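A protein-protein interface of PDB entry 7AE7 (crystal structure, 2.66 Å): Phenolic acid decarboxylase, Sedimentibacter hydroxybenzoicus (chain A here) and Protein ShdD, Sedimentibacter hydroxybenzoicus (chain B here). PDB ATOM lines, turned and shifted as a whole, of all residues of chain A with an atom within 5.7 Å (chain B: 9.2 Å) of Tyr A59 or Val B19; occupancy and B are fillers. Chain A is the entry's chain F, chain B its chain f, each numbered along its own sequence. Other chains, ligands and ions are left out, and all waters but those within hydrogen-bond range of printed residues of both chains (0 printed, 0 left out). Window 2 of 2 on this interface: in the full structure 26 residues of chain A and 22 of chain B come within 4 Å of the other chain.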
ATOM      1  N   PRO A  30      -4.203 -18.129 -13.168  1.00  0.00           N
ATOM      2  CA  PRO A  30      -5.038 -18.306 -11.963  1.00  0.00           C
ATOM      3  C   PRO A  30      -6.459 -18.751 -12.269  1.00  0.00           C
ATOM      4  O   PRO A  30      -6.998 -19.615 -11.564  1.00  0.00           O
ATOM      5  CB  PRO A  30      -5.008 -16.919 -11.303  1.00  0.00           C
ATOM      6  CG  PRO A  30      -3.838 -16.210 -11.910  1.00  0.00           C
ATOM      7  CD  PRO A  30      -3.657 -16.767 -13.283  1.00  0.00           C
ATOM      8  N   GLU A  31      -7.078 -18.198 -13.313  1.00  0.00           N
ATOM      9  CA  GLU A  31      -8.417 -18.587 -13.719  1.00  0.00           C
ATOM     10  C   GLU A  31      -8.421 -19.005 -15.183  1.00  0.00           C
ATOM     11  O   GLU A  31      -7.815 -18.328 -16.021  1.00  0.00           O
ATOM     12  CB  GLU A  31      -9.425 -17.443 -13.525  1.00  0.00           C
ATOM     13  CG  GLU A  31      -9.494 -16.879 -12.115  1.00  0.00           C
ATOM     14  CD  GLU A  31      -8.503 -15.754 -11.888  1.00  0.00           C
ATOM     15  OE1 GLU A  31      -8.117 -15.092 -12.876  1.00  0.00           O
ATOM     16  OE2 GLU A  31      -8.120 -15.523 -10.723  1.00  0.00           O
ATOM     17  N   ILE A  56       2.239 -20.104 -10.839  1.00  0.00           N
ATOM     18  CA  ILE A  56       1.009 -19.426 -11.233  1.00  0.00           C
ATOM     19  C   ILE A  56       1.387 -18.036 -11.724  1.00  0.00           C
ATOM     20  O   ILE A  56       2.098 -17.304 -11.027  1.00  0.00           O
ATOM     21  CB  ILE A  56       0.009 -19.346 -10.066  1.00  0.00           C
ATOM     22  CG1 ILE A  56      -0.236 -20.740  -9.482  1.00  0.00           C
ATOM     23  CG2 ILE A  56      -1.297 -18.715 -10.524  1.00  0.00           C
ATOM     24  CD1 ILE A  56       0.423 -20.966  -8.140  1.00  0.00           C
ATOM     25  N   LYS A  57       0.915 -17.679 -12.920  1.00  0.00           N
ATOM     26  CA  LYS A  57       1.356 -16.445 -13.563  1.00  0.00           C
ATOM     27  C   LYS A  57       1.064 -15.230 -12.692  1.00  0.00           C
ATOM     28  O   LYS A  57      -0.057 -15.052 -12.205  1.00  0.00           O
ATOM     29  CB  LYS A  57       0.684 -16.278 -14.926  1.00  0.00           C
ATOM     30  CG  LYS A  57       1.340 -15.204 -15.788  1.00  0.00           C
ATOM     31  CD  LYS A  57       0.998 -15.361 -17.263  1.00  0.00           C
ATOM     32  CE  LYS A  57      -0.483 -15.126 -17.524  1.00  0.00           C
ATOM     33  NZ  LYS A  57      -0.711 -14.051 -18.531  1.00  0.00           N
ATOM     34  N   GLY A  58       2.082 -14.392 -12.503  1.00  0.00           N
ATOM     35  CA  GLY A  58       1.955 -13.186 -11.716  1.00  0.00           C
ATOM     36  C   GLY A  58       2.201 -13.354 -10.233  1.00  0.00           C
ATOM     37  O   GLY A  58       2.413 -12.349  -9.543  1.00  0.00           O
ATOM     38  N   TYR A  59       2.199 -14.581  -9.722  1.00  0.00           N
ATOM     39  CA  TYR A  59       2.364 -14.841  -8.302  1.00  0.00           C
ATOM     40  C   TYR A  59       3.727 -15.467  -8.028  1.00  0.00           C
ATOM     41  O   TYR A  59       4.370 -16.034  -8.915  1.00  0.00           O
ATOM     42  CB  TYR A  59       1.251 -15.758  -7.780  1.00  0.00           C
ATOM     43  CG  TYR A  59      -0.117 -15.113  -7.756  1.00  0.00           C
ATOM     44  CD1 TYR A  59      -0.398 -14.063  -6.892  1.00  0.00           C
ATOM     45  CD2 TYR A  59      -1.132 -15.561  -8.595  1.00  0.00           C
ATOM     46  CE1 TYR A  59      -1.650 -13.475  -6.865  1.00  0.00           C
ATOM     47  CE2 TYR A  59      -2.387 -14.979  -8.574  1.00  0.00           C
ATOM     48  CZ  TYR A  59      -2.641 -13.938  -7.707  1.00  0.00           C
ATOM     49  OH  TYR A  59      -3.885 -13.350  -7.680  1.00  0.00           O
ATOM     50  N   LYS A  60       4.157 -15.359  -6.771  1.00  0.00           N
ATOM     51  CA  LYS A  60       5.481 -15.812  -6.368  1.00  0.00           C
ATOM     52  C   LYS A  60       5.496 -17.226  -5.799  1.00  0.00           C
ATOM     53  O   LYS A  60       6.541 -17.885  -5.849  1.00  0.00           O
ATOM     54  CB  LYS A  60       6.069 -14.847  -5.331  1.00  0.00           C
ATOM     55  CG  LYS A  60       7.545 -15.062  -5.025  1.00  0.00           C
ATOM     56  CD  LYS A  60       8.270 -13.743  -4.801  1.00  0.00           C
ATOM     57  CE  LYS A  60       9.363 -13.883  -3.748  1.00  0.00           C
ATOM     58  NZ  LYS A  60       9.549 -12.631  -2.964  1.00  0.00           N
ATOM     59  N   TYR A  61       4.377 -17.715  -5.274  1.00  0.00           N
ATOM     60  CA  TYR A  61       4.367 -18.953  -4.504  1.00  0.00           C
ATOM     61  C   TYR A  61       3.413 -19.979  -5.122  1.00  0.00           C
ATOM     62  O   TYR A  61       2.885 -19.792  -6.222  1.00  0.00           O
ATOM     63  CB  TYR A  61       4.037 -18.646  -3.042  1.00  0.00           C
ATOM     64  CG  TYR A  61       5.077 -17.752  -2.411  1.00  0.00           C
ATOM     65  CD1 TYR A  61       6.424 -18.086  -2.473  1.00  0.00           C
ATOM     66  CD2 TYR A  61       4.723 -16.571  -1.778  1.00  0.00           C
ATOM     67  CE1 TYR A  61       7.387 -17.278  -1.911  1.00  0.00           C
ATOM     68  CE2 TYR A  61       5.681 -15.752  -1.212  1.00  0.00           C
ATOM     69  CZ  TYR A  61       7.013 -16.111  -1.283  1.00  0.00           C
ATOM     70  OH  TYR A  61       7.975 -15.303  -0.722  1.00  0.00           O
ATOM     71  N   PHE A 126      -2.151 -10.553  -1.806  1.00  0.00           N
ATOM     72  CA  PHE A 126      -1.758 -11.079  -3.107  1.00  0.00           C
ATOM     73  C   PHE A 126      -0.254 -11.290  -3.219  1.00  0.00           C
ATOM     74  O   PHE A 126       0.185 -12.087  -4.055  1.00  0.00           O
ATOM     75  CB  PHE A 126      -2.244 -10.147  -4.216  1.00  0.00           C
ATOM     76  CG  PHE A 126      -3.739 -10.041  -4.299  1.00  0.00           C
ATOM     77  CD1 PHE A 126      -4.439  -9.214  -3.436  1.00  0.00           C
ATOM     78  CD2 PHE A 126      -4.446 -10.773  -5.237  1.00  0.00           C
ATOM     79  CE1 PHE A 126      -5.815  -9.117  -3.509  1.00  0.00           C
ATOM     80  CE2 PHE A 126      -5.822 -10.682  -5.316  1.00  0.00           C
ATOM     81  CZ  PHE A 126      -6.507  -9.852  -4.451  1.00  0.00           C
ATOM     82  N   LEU A 129      -0.505 -15.111  -1.026  1.00  0.00           N
ATOM     83  CA  LEU A 129      -1.344 -16.189  -1.542  1.00  0.00           C
ATOM     84  C   LEU A 129      -1.644 -15.973  -3.019  1.00  0.00           C
ATOM     85  O   LEU A 129      -2.050 -14.871  -3.409  1.00  0.00           O
ATOM     86  CB  LEU A 129      -2.647 -16.289  -0.761  1.00  0.00           C
ATOM     87  CG  LEU A 129      -2.526 -16.114   0.752  1.00  0.00           C
ATOM     88  CD1 LEU A 129      -3.843 -15.639   1.340  1.00  0.00           C
ATOM     89  CD2 LEU A 129      -2.074 -17.410   1.411  1.00  0.00           C
ATOM     90  N   PRO A 130      -1.437 -16.975  -3.865  1.00  0.00           N
ATOM     91  CA  PRO A 130      -1.889 -16.857  -5.256  1.00  0.00           C
ATOM     92  C   PRO A 130      -3.403 -16.961  -5.360  1.00  0.00           C
ATOM     93  O   PRO A 130      -3.930 -18.022  -5.710  1.00  0.00           O
ATOM     94  CB  PRO A 130      -1.197 -18.033  -5.954  1.00  0.00           C
ATOM     95  CG  PRO A 130      -0.074 -18.417  -5.047  1.00  0.00           C
ATOM     96  CD  PRO A 130      -0.579 -18.152  -3.664  1.00  0.00           C
ATOM     97  N   LEU A 131      -4.104 -15.870  -5.053  1.00  0.00           N
ATOM     98  CA  LEU A 131      -5.560 -15.887  -5.026  1.00  0.00           C
ATOM     99  C   LEU A 131      -6.136 -15.999  -6.433  1.00  0.00           C
ATOM    100  O   LEU A 131      -5.599 -15.441  -7.393  1.00  0.00           O
ATOM    101  CB  LEU A 131      -6.087 -14.630  -4.336  1.00  0.00           C
ATOM    102  CG  LEU A 131      -5.640 -14.462  -2.884  1.00  0.00           C
ATOM    103  CD1 LEU A 131      -5.593 -12.991  -2.494  1.00  0.00           C
ATOM    104  CD2 LEU A 131      -6.549 -15.241  -1.946  1.00  0.00           C
ATOM    105  N   TYR A 132      -7.243 -16.729  -6.544  1.00  0.00           N
ATOM    106  CA  TYR A 132      -7.894 -16.983  -7.819  1.00  0.00           C
ATOM    107  C   TYR A 132      -9.389 -17.112  -7.571  1.00  0.00           C
ATOM    108  O   TYR A 132      -9.844 -17.173  -6.425  1.00  0.00           O
ATOM    109  CB  TYR A 132      -7.342 -18.247  -8.490  1.00  0.00           C
ATOM    110  CG  TYR A 132      -7.516 -19.500  -7.659  1.00  0.00           C
ATOM    111  CD1 TYR A 132      -6.643 -19.798  -6.621  1.00  0.00           C
ATOM    112  CD2 TYR A 132      -8.561 -20.380  -7.909  1.00  0.00           C
ATOM    113  CE1 TYR A 132      -6.802 -20.938  -5.860  1.00  0.00           C
ATOM    114  CE2 TYR A 132      -8.728 -21.523  -7.153  1.00  0.00           C
ATOM    115  CZ  TYR A 132      -7.846 -21.795  -6.129  1.00  0.00           C
ATOM    116  OH  TYR A 132      -8.005 -22.933  -5.372  1.00  0.00           O
ATOM    117  N   PHE A 141     -12.255 -13.427  -5.109  1.00  0.00           N
ATOM    118  CA  PHE A 141     -11.294 -14.473  -4.792  1.00  0.00           C
ATOM    119  C   PHE A 141     -11.481 -14.892  -3.340  1.00  0.00           C
ATOM    120  O   PHE A 141     -11.564 -14.041  -2.448  1.00  0.00           O
ATOM    121  CB  PHE A 141      -9.863 -13.992  -5.037  1.00  0.00           C
ATOM    122  CG  PHE A 141      -9.639 -13.424  -6.413  1.00  0.00           C
ATOM    123  CD1 PHE A 141     -10.406 -13.842  -7.491  1.00  0.00           C
ATOM    124  CD2 PHE A 141      -8.660 -12.469  -6.628  1.00  0.00           C
ATOM    125  CE1 PHE A 141     -10.201 -13.316  -8.753  1.00  0.00           C
ATOM    126  CE2 PHE A 141      -8.449 -11.942  -7.889  1.00  0.00           C
ATOM    127  CZ  PHE A 141      -9.221 -12.366  -8.953  1.00  0.00           C
ATOM    128  N   MET B  14      -7.458  -2.749  -7.428  1.00  0.00           N
ATOM    129  CA  MET B  14      -7.067  -3.280  -6.129  1.00  0.00           C
ATOM    130  C   MET B  14      -5.554  -3.430  -6.026  1.00  0.00           C
ATOM    131  O   MET B  14      -4.906  -2.756  -5.218  1.00  0.00           O
ATOM    132  CB  MET B  14      -7.761  -4.621  -5.882  1.00  0.00           C
ATOM    133  CG  MET B  14      -8.257  -4.800  -4.461  1.00  0.00           C
ATOM    134  SD  MET B  14      -8.333  -6.532  -3.977  1.00  0.00           S
ATOM    135  CE  MET B  14      -9.858  -7.031  -4.766  1.00  0.00           C
ATOM    136  N   VAL B  15      -4.973  -4.305  -6.850  1.00  0.00           N
ATOM    137  CA  VAL B  15      -3.540  -4.575  -6.822  1.00  0.00           C
ATOM    138  C   VAL B  15      -3.054  -4.859  -8.237  1.00  0.00           C
ATOM    139  O   VAL B  15      -3.832  -5.198  -9.137  1.00  0.00           O
ATOM    140  CB  VAL B  15      -3.165  -5.768  -5.903  1.00  0.00           C
ATOM    141  CG1 VAL B  15      -3.644  -5.553  -4.471  1.00  0.00           C
ATOM    142  CG2 VAL B  15      -3.720  -7.070  -6.468  1.00  0.00           C
ATOM    143  N   ASP B  16      -1.748  -4.713  -8.426  1.00  0.00           N
ATOM    144  CA  ASP B  16      -1.046  -5.189  -9.606  1.00  0.00           C
ATOM    145  C   ASP B  16      -0.460  -6.565  -9.320  1.00  0.00           C
ATOM    146  O   ASP B  16      -0.244  -6.945  -8.165  1.00  0.00           O
ATOM    147  CB  ASP B  16       0.067  -4.219 -10.012  1.00  0.00           C
ATOM    148  CG  ASP B  16      -0.468  -2.901 -10.534  1.00  0.00           C
ATOM    149  OD1 ASP B  16      -0.878  -2.845 -11.712  1.00  0.00           O
ATOM    150  OD2 ASP B  16      -0.474  -1.916  -9.767  1.00  0.00           O
ATOM    151  N   SER B  17      -0.209  -7.313 -10.388  1.00  0.00           N
ATOM    152  CA  SER B  17       0.392  -8.630 -10.240  1.00  0.00           C
ATOM    153  C   SER B  17       1.747  -8.498  -9.550  1.00  0.00           C
ATOM    154  O   SER B  17       2.594  -7.718 -10.007  1.00  0.00           O
ATOM    155  CB  SER B  17       0.555  -9.304 -11.602  1.00  0.00           C
ATOM    156  OG  SER B  17       1.462  -8.582 -12.414  1.00  0.00           O
ATOM    157  N   PRO B  18       1.983  -9.219  -8.451  1.00  0.00           N
ATOM    158  CA  PRO B  18       3.254  -9.058  -7.727  1.00  0.00           C
ATOM    159  C   PRO B  18       4.481  -9.346  -8.572  1.00  0.00           C
ATOM    160  O   PRO B  18       5.526  -8.717  -8.363  1.00  0.00           O
ATOM    161  CB  PRO B  18       3.119 -10.056  -6.568  1.00  0.00           C
ATOM    162  CG  PRO B  18       1.646 -10.203  -6.370  1.00  0.00           C
ATOM    163  CD  PRO B  18       1.044 -10.103  -7.740  1.00  0.00           C
ATOM    164  N   VAL B  19       4.391 -10.272  -9.521  1.00  0.00           N
ATOM    165  CA  VAL B  19       5.509 -10.632 -10.386  1.00  0.00           C
ATOM    166  C   VAL B  19       5.183 -10.178 -11.802  1.00  0.00           C
ATOM    167  O   VAL B  19       4.159 -10.579 -12.369  1.00  0.00           O
ATOM    168  CB  VAL B  19       5.796 -12.140 -10.345  1.00  0.00           C
ATOM    169  CG1 VAL B  19       6.929 -12.491 -11.299  1.00  0.00           C
ATOM    170  CG2 VAL B  19       6.124 -12.576  -8.926  1.00  0.00           C
ATOM    171  N   GLY B  20       6.051  -9.344 -12.368  1.00  0.00           N
ATOM    172  CA  GLY B  20       5.870  -8.912 -13.738  1.00  0.00           C
ATOM    173  C   GLY B  20       4.656  -8.012 -13.923  1.00  0.00           C
ATOM    174  O   GLY B  20       4.094  -7.453 -12.977  1.00  0.00           O
ATOM    175  N   ASP B  21       4.252  -7.887 -15.187  1.00  0.00           N
ATOM    176  CA  ASP B  21       3.127  -7.041 -15.567  1.00  0.00           C
ATOM    177  C   ASP B  21       2.013  -7.881 -16.179  1.00  0.00           C
ATOM    178  O   ASP B  21       1.457  -7.522 -17.223  1.00  0.00           O
ATOM    179  CB  ASP B  21       3.579  -5.956 -16.547  1.00  0.00           C
ATOM    180  CG  ASP B  21       4.144  -4.735 -15.844  1.00  0.00           C
ATOM    181  OD1 ASP B  21       5.294  -4.800 -15.360  1.00  0.00           O
ATOM    182  OD2 ASP B  21       3.435  -3.707 -15.779  1.00  0.00           O
ATOM    183  N   ALA B  22       1.695  -9.011 -15.543  1.00  0.00           N
ATOM    184  CA  ALA B  22       0.794  -9.989 -16.144  1.00  0.00           C
ATOM    185  C   ALA B  22      -0.672  -9.567 -16.076  1.00  0.00           C
ATOM    186  O   ALA B  22      -1.419  -9.784 -17.036  1.00  0.00           O
ATOM    187  CB  ALA B  22       0.984 -11.351 -15.474  1.00  0.00           C
ATOM    188  N   TRP B  23      -1.113  -8.977 -14.965  1.00  0.00           N
ATOM    189  CA  TRP B  23      -2.531  -8.664 -14.813  1.00  0.00           C
ATOM    190  C   TRP B  23      -2.717  -7.588 -13.749  1.00  0.00           C
ATOM    191  O   TRP B  23      -1.761  -7.113 -13.132  1.00  0.00           O
ATOM    192  CB  TRP B  23      -3.343  -9.917 -14.467  1.00  0.00           C
ATOM    193  CG  TRP B  23      -2.689 -10.824 -13.465  1.00  0.00           C
ATOM    194  CD1 TRP B  23      -2.010 -11.977 -13.727  1.00  0.00           C
ATOM    195  CD2 TRP B  23      -2.666 -10.660 -12.040  1.00  0.00           C
ATOM    196  NE1 TRP B  23      -1.559 -12.538 -12.557  1.00  0.00           N
ATOM    197  CE2 TRP B  23      -1.949 -11.749 -11.507  1.00  0.00           C
ATOM    198  CE3 TRP B  23      -3.178  -9.698 -11.165  1.00  0.00           C
ATOM    199  CZ2 TRP B  23      -1.730 -11.902 -10.140  1.00  0.00           C
ATOM    200  CZ3 TRP B  23      -2.960  -9.852  -9.807  1.00  0.00           C
ATOM    201  CH2 TRP B  23      -2.242 -10.945  -9.309  1.00  0.00           C
ATOM    202  N   GLU B  24      -3.980  -7.209 -13.551  1.00  0.00           N
ATOM    203  CA  GLU B  24      -4.405  -6.263 -12.530  1.00  0.00           C
ATOM    204  C   GLU B  24      -5.731  -6.750 -11.964  1.00  0.00           C
ATOM    205  O   GLU B  24      -6.487  -7.443 -12.647  1.00  0.00           O
ATOM    206  CB  GLU B  24      -4.567  -4.846 -13.101  1.00  0.00           C
ATOM    207  CG  GLU B  24      -3.265  -4.170 -13.499  1.00  0.00           C
ATOM    208  CD  GLU B  24      -2.959  -4.316 -14.980  1.00  0.00           C
ATOM    209  OE1 GLU B  24      -3.888  -4.159 -15.802  1.00  0.00           O
ATOM    210  OE2 GLU B  24      -1.790  -4.593 -15.323  1.00  0.00           O
ATOM    211  N   VAL B  25      -6.016  -6.388 -10.715  1.00  0.00           N
ATOM    212  CA  VAL B  25      -7.270  -6.768 -10.072  1.00  0.00           C
ATOM    213  C   VAL B  25      -8.089  -5.507  -9.838  1.00  0.00           C
ATOM    214  O   VAL B  25      -7.615  -4.556  -9.203  1.00  0.00           O
ATOM    215  CB  VAL B  25      -7.035  -7.530  -8.758  1.00  0.00           C
ATOM    216  CG1 VAL B  25      -8.359  -7.780  -8.055  1.00  0.00           C
ATOM    217  CG2 VAL B  25      -6.324  -8.845  -9.029  1.00  0.00           C
ATOM    218  N   TRP B  35     -12.542  -8.599  -9.966  1.00  0.00           N
ATOM    219  CA  TRP B  35     -12.221  -9.447 -11.105  1.00  0.00           C
ATOM    220  C   TRP B  35     -10.821  -9.121 -11.605  1.00  0.00           C
ATOM    221  O   TRP B  35     -10.263  -8.062 -11.308  1.00  0.00           O
ATOM    222  CB  TRP B  35     -13.252  -9.296 -12.229  1.00  0.00           C
ATOM    223  CG  TRP B  35     -13.198  -7.981 -12.933  1.00  0.00           C
ATOM    224  CD1 TRP B  35     -12.577  -7.710 -14.117  1.00  0.00           C
ATOM    225  CD2 TRP B  35     -13.795  -6.752 -12.502  1.00  0.00           C
ATOM    226  NE1 TRP B  35     -12.747  -6.388 -14.449  1.00  0.00           N
ATOM    227  CE2 TRP B  35     -13.492  -5.778 -13.474  1.00  0.00           C
ATOM    228  CE3 TRP B  35     -14.554  -6.380 -11.388  1.00  0.00           C
ATOM    229  CZ2 TRP B  35     -13.921  -4.456 -13.365  1.00  0.00           C
ATOM    230  CZ3 TRP B  35     -14.979  -5.066 -11.283  1.00  0.00           C
ATOM    231  CH2 TRP B  35     -14.661  -4.121 -12.265  1.00  0.00           C
ATOM    232  N   ARG B  36     -10.259 -10.051 -12.369  1.00  0.00           N
ATOM    233  CA  ARG B  36      -8.910  -9.899 -12.890  1.00  0.00           C
ATOM    234  C   ARG B  36      -8.938  -9.332 -14.303  1.00  0.00           C
ATOM    235  O   ARG B  36      -9.896  -9.524 -15.057  1.00  0.00           O
ATOM    236  CB  ARG B  36      -8.156 -11.230 -12.880  1.00  0.00           C
ATOM    237  CG  ARG B  36      -6.651 -11.059 -12.720  1.00  0.00           C
ATOM    238  CD  ARG B  36      -5.910 -12.380 -12.834  1.00  0.00           C
ATOM    239  NE  ARG B  36      -6.340 -13.333 -11.819  1.00  0.00           N
ATOM    240  CZ  ARG B  36      -5.880 -13.361 -10.576  1.00  0.00           C
ATOM    241  NH1 ARG B  36      -4.968 -12.500 -10.158  1.00  0.00           N
ATOM    242  NH2 ARG B  36      -6.349 -14.274  -9.731  1.00  0.00           N
ATOM    243  N   THR B  38      -7.245 -10.270 -16.813  1.00  0.00           N
ATOM    244  CA  THR B  38      -7.144 -11.302 -17.837  1.00  0.00           C
ATOM    245  C   THR B  38      -8.420 -12.114 -18.014  1.00  0.00           C
ATOM    246  O   THR B  38      -8.545 -12.819 -19.022  1.00  0.00           O
ATOM    247  CB  THR B  38      -5.980 -12.247 -17.523  1.00  0.00           C
ATOM    248  OG1 THR B  38      -5.881 -12.433 -16.105  1.00  0.00           O
ATOM    249  CG2 THR B  38      -4.672 -11.677 -18.051  1.00  0.00           C
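The side-chain hydroxyl of Ser B17 sits at hydrogen-bond distance from the backbone NH of Ala B22, 3.2 Å away.
The backbone carbonyl oxygen (O) of Val B19 lies within hydrogen-bond range of the side-chain hydroxyl (OG) of Ser B17 (3.4 Å).
The backbone NH (N) of Ser B17 sits at hydrogen-bond distance from the backbone carbonyl oxygen (O) of Trp B23, at 3.2 Å.
N of Val B25 lies within hydrogen-bond range of O of Val B15.
N of Met B14 lies within hydrogen-bond range of O of Val B25, at 2.5 Å.
OH of Tyr A59 lies within hydrogen-bond range of O of Leu A131, 2.7 Å away.
Of the 15 printed residues of chain B, 9 touch a printed residue of chain A.
Hydrophobic or aromatic side chains of chain B within 4 Å of the printed part of chain A: Met B14, Val B15, Pro B18, Val B19, Ala B22, Trp B23 and Val B25.
Of the 14 printed residues of chain A, 9 touch a printed residue of chain B.
Among the printed residues, 18 pairs touch across the chains.
OE1 of Glu A31 is in salt-bridge range of NE of Arg B36, 2.7 Å away.
O of Gly A58 lies close to N of Pro B18.
O of Leu A131 sits at hydrogen-bond distance from NH2 of Arg B36 (2.7 Å).
The backbone carbonyl oxygen of Lys A57 is in hydrogen-bond range of the indole nitrogen of Trp B23 (2.9 Å).
NH1 of Arg B36 sits at hydrogen-bond distance from OH of Tyr A59 (2.8 Å).
O of Gly A58 sits at hydrogen-bond distance from N of Val B19, at 2.9 Å.
Of chain B, only Val B19, Trp B23 and Arg B36 come within 4 Å of Tyr A59.
Of chain A, only Gly A58 (2.9 Å) and Tyr A59 (3.9 Å) come within 4 Å of Val B19.
No residue of chain B comes within 4 Å of Pro A130.
Of the printed residues of chain A, Ala B22 touches Lys A57.
Printed residues of chain B within 4 Å of Leu A131: Arg B36 (2.7 Å).
Of the printed residues of chain B, Phe A141 touches Val B25 and Arg B36.
Of the printed residues of chain A, Pro B18 touches Gly A58 (3.2 Å) and Phe A126 (3.3 Å).
Printed residues of chain B within 4 Å of Phe A126: Met B14 (3.6 Å), Val B15 (3.7 Å) and Pro B18 (3.3 Å).
Arg B36 touches Pro A30.
CB of Ala B22 touches CG of Lys A57 (3.9 Å).
CA of Gly A58 touches NE1 of Trp B23, at 3.7 Å.
Val B19 touches Tyr A59 (CG2 to C, 3.9 Å).
CZ2 of Trp B23 touches CZ of Tyr A59, at 3.3 Å.
SD of Met B14 touches CE1 of Phe A126, at 3.6 Å.
CG of Phe A126 touches CG2 of Val B15, at 3.7 Å.
Arg B36 touches Tyr A132.
Phe A141 touches Val B25.
NH2 of Arg B36 touches CZ of Phe A141, 3.5 Å away.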
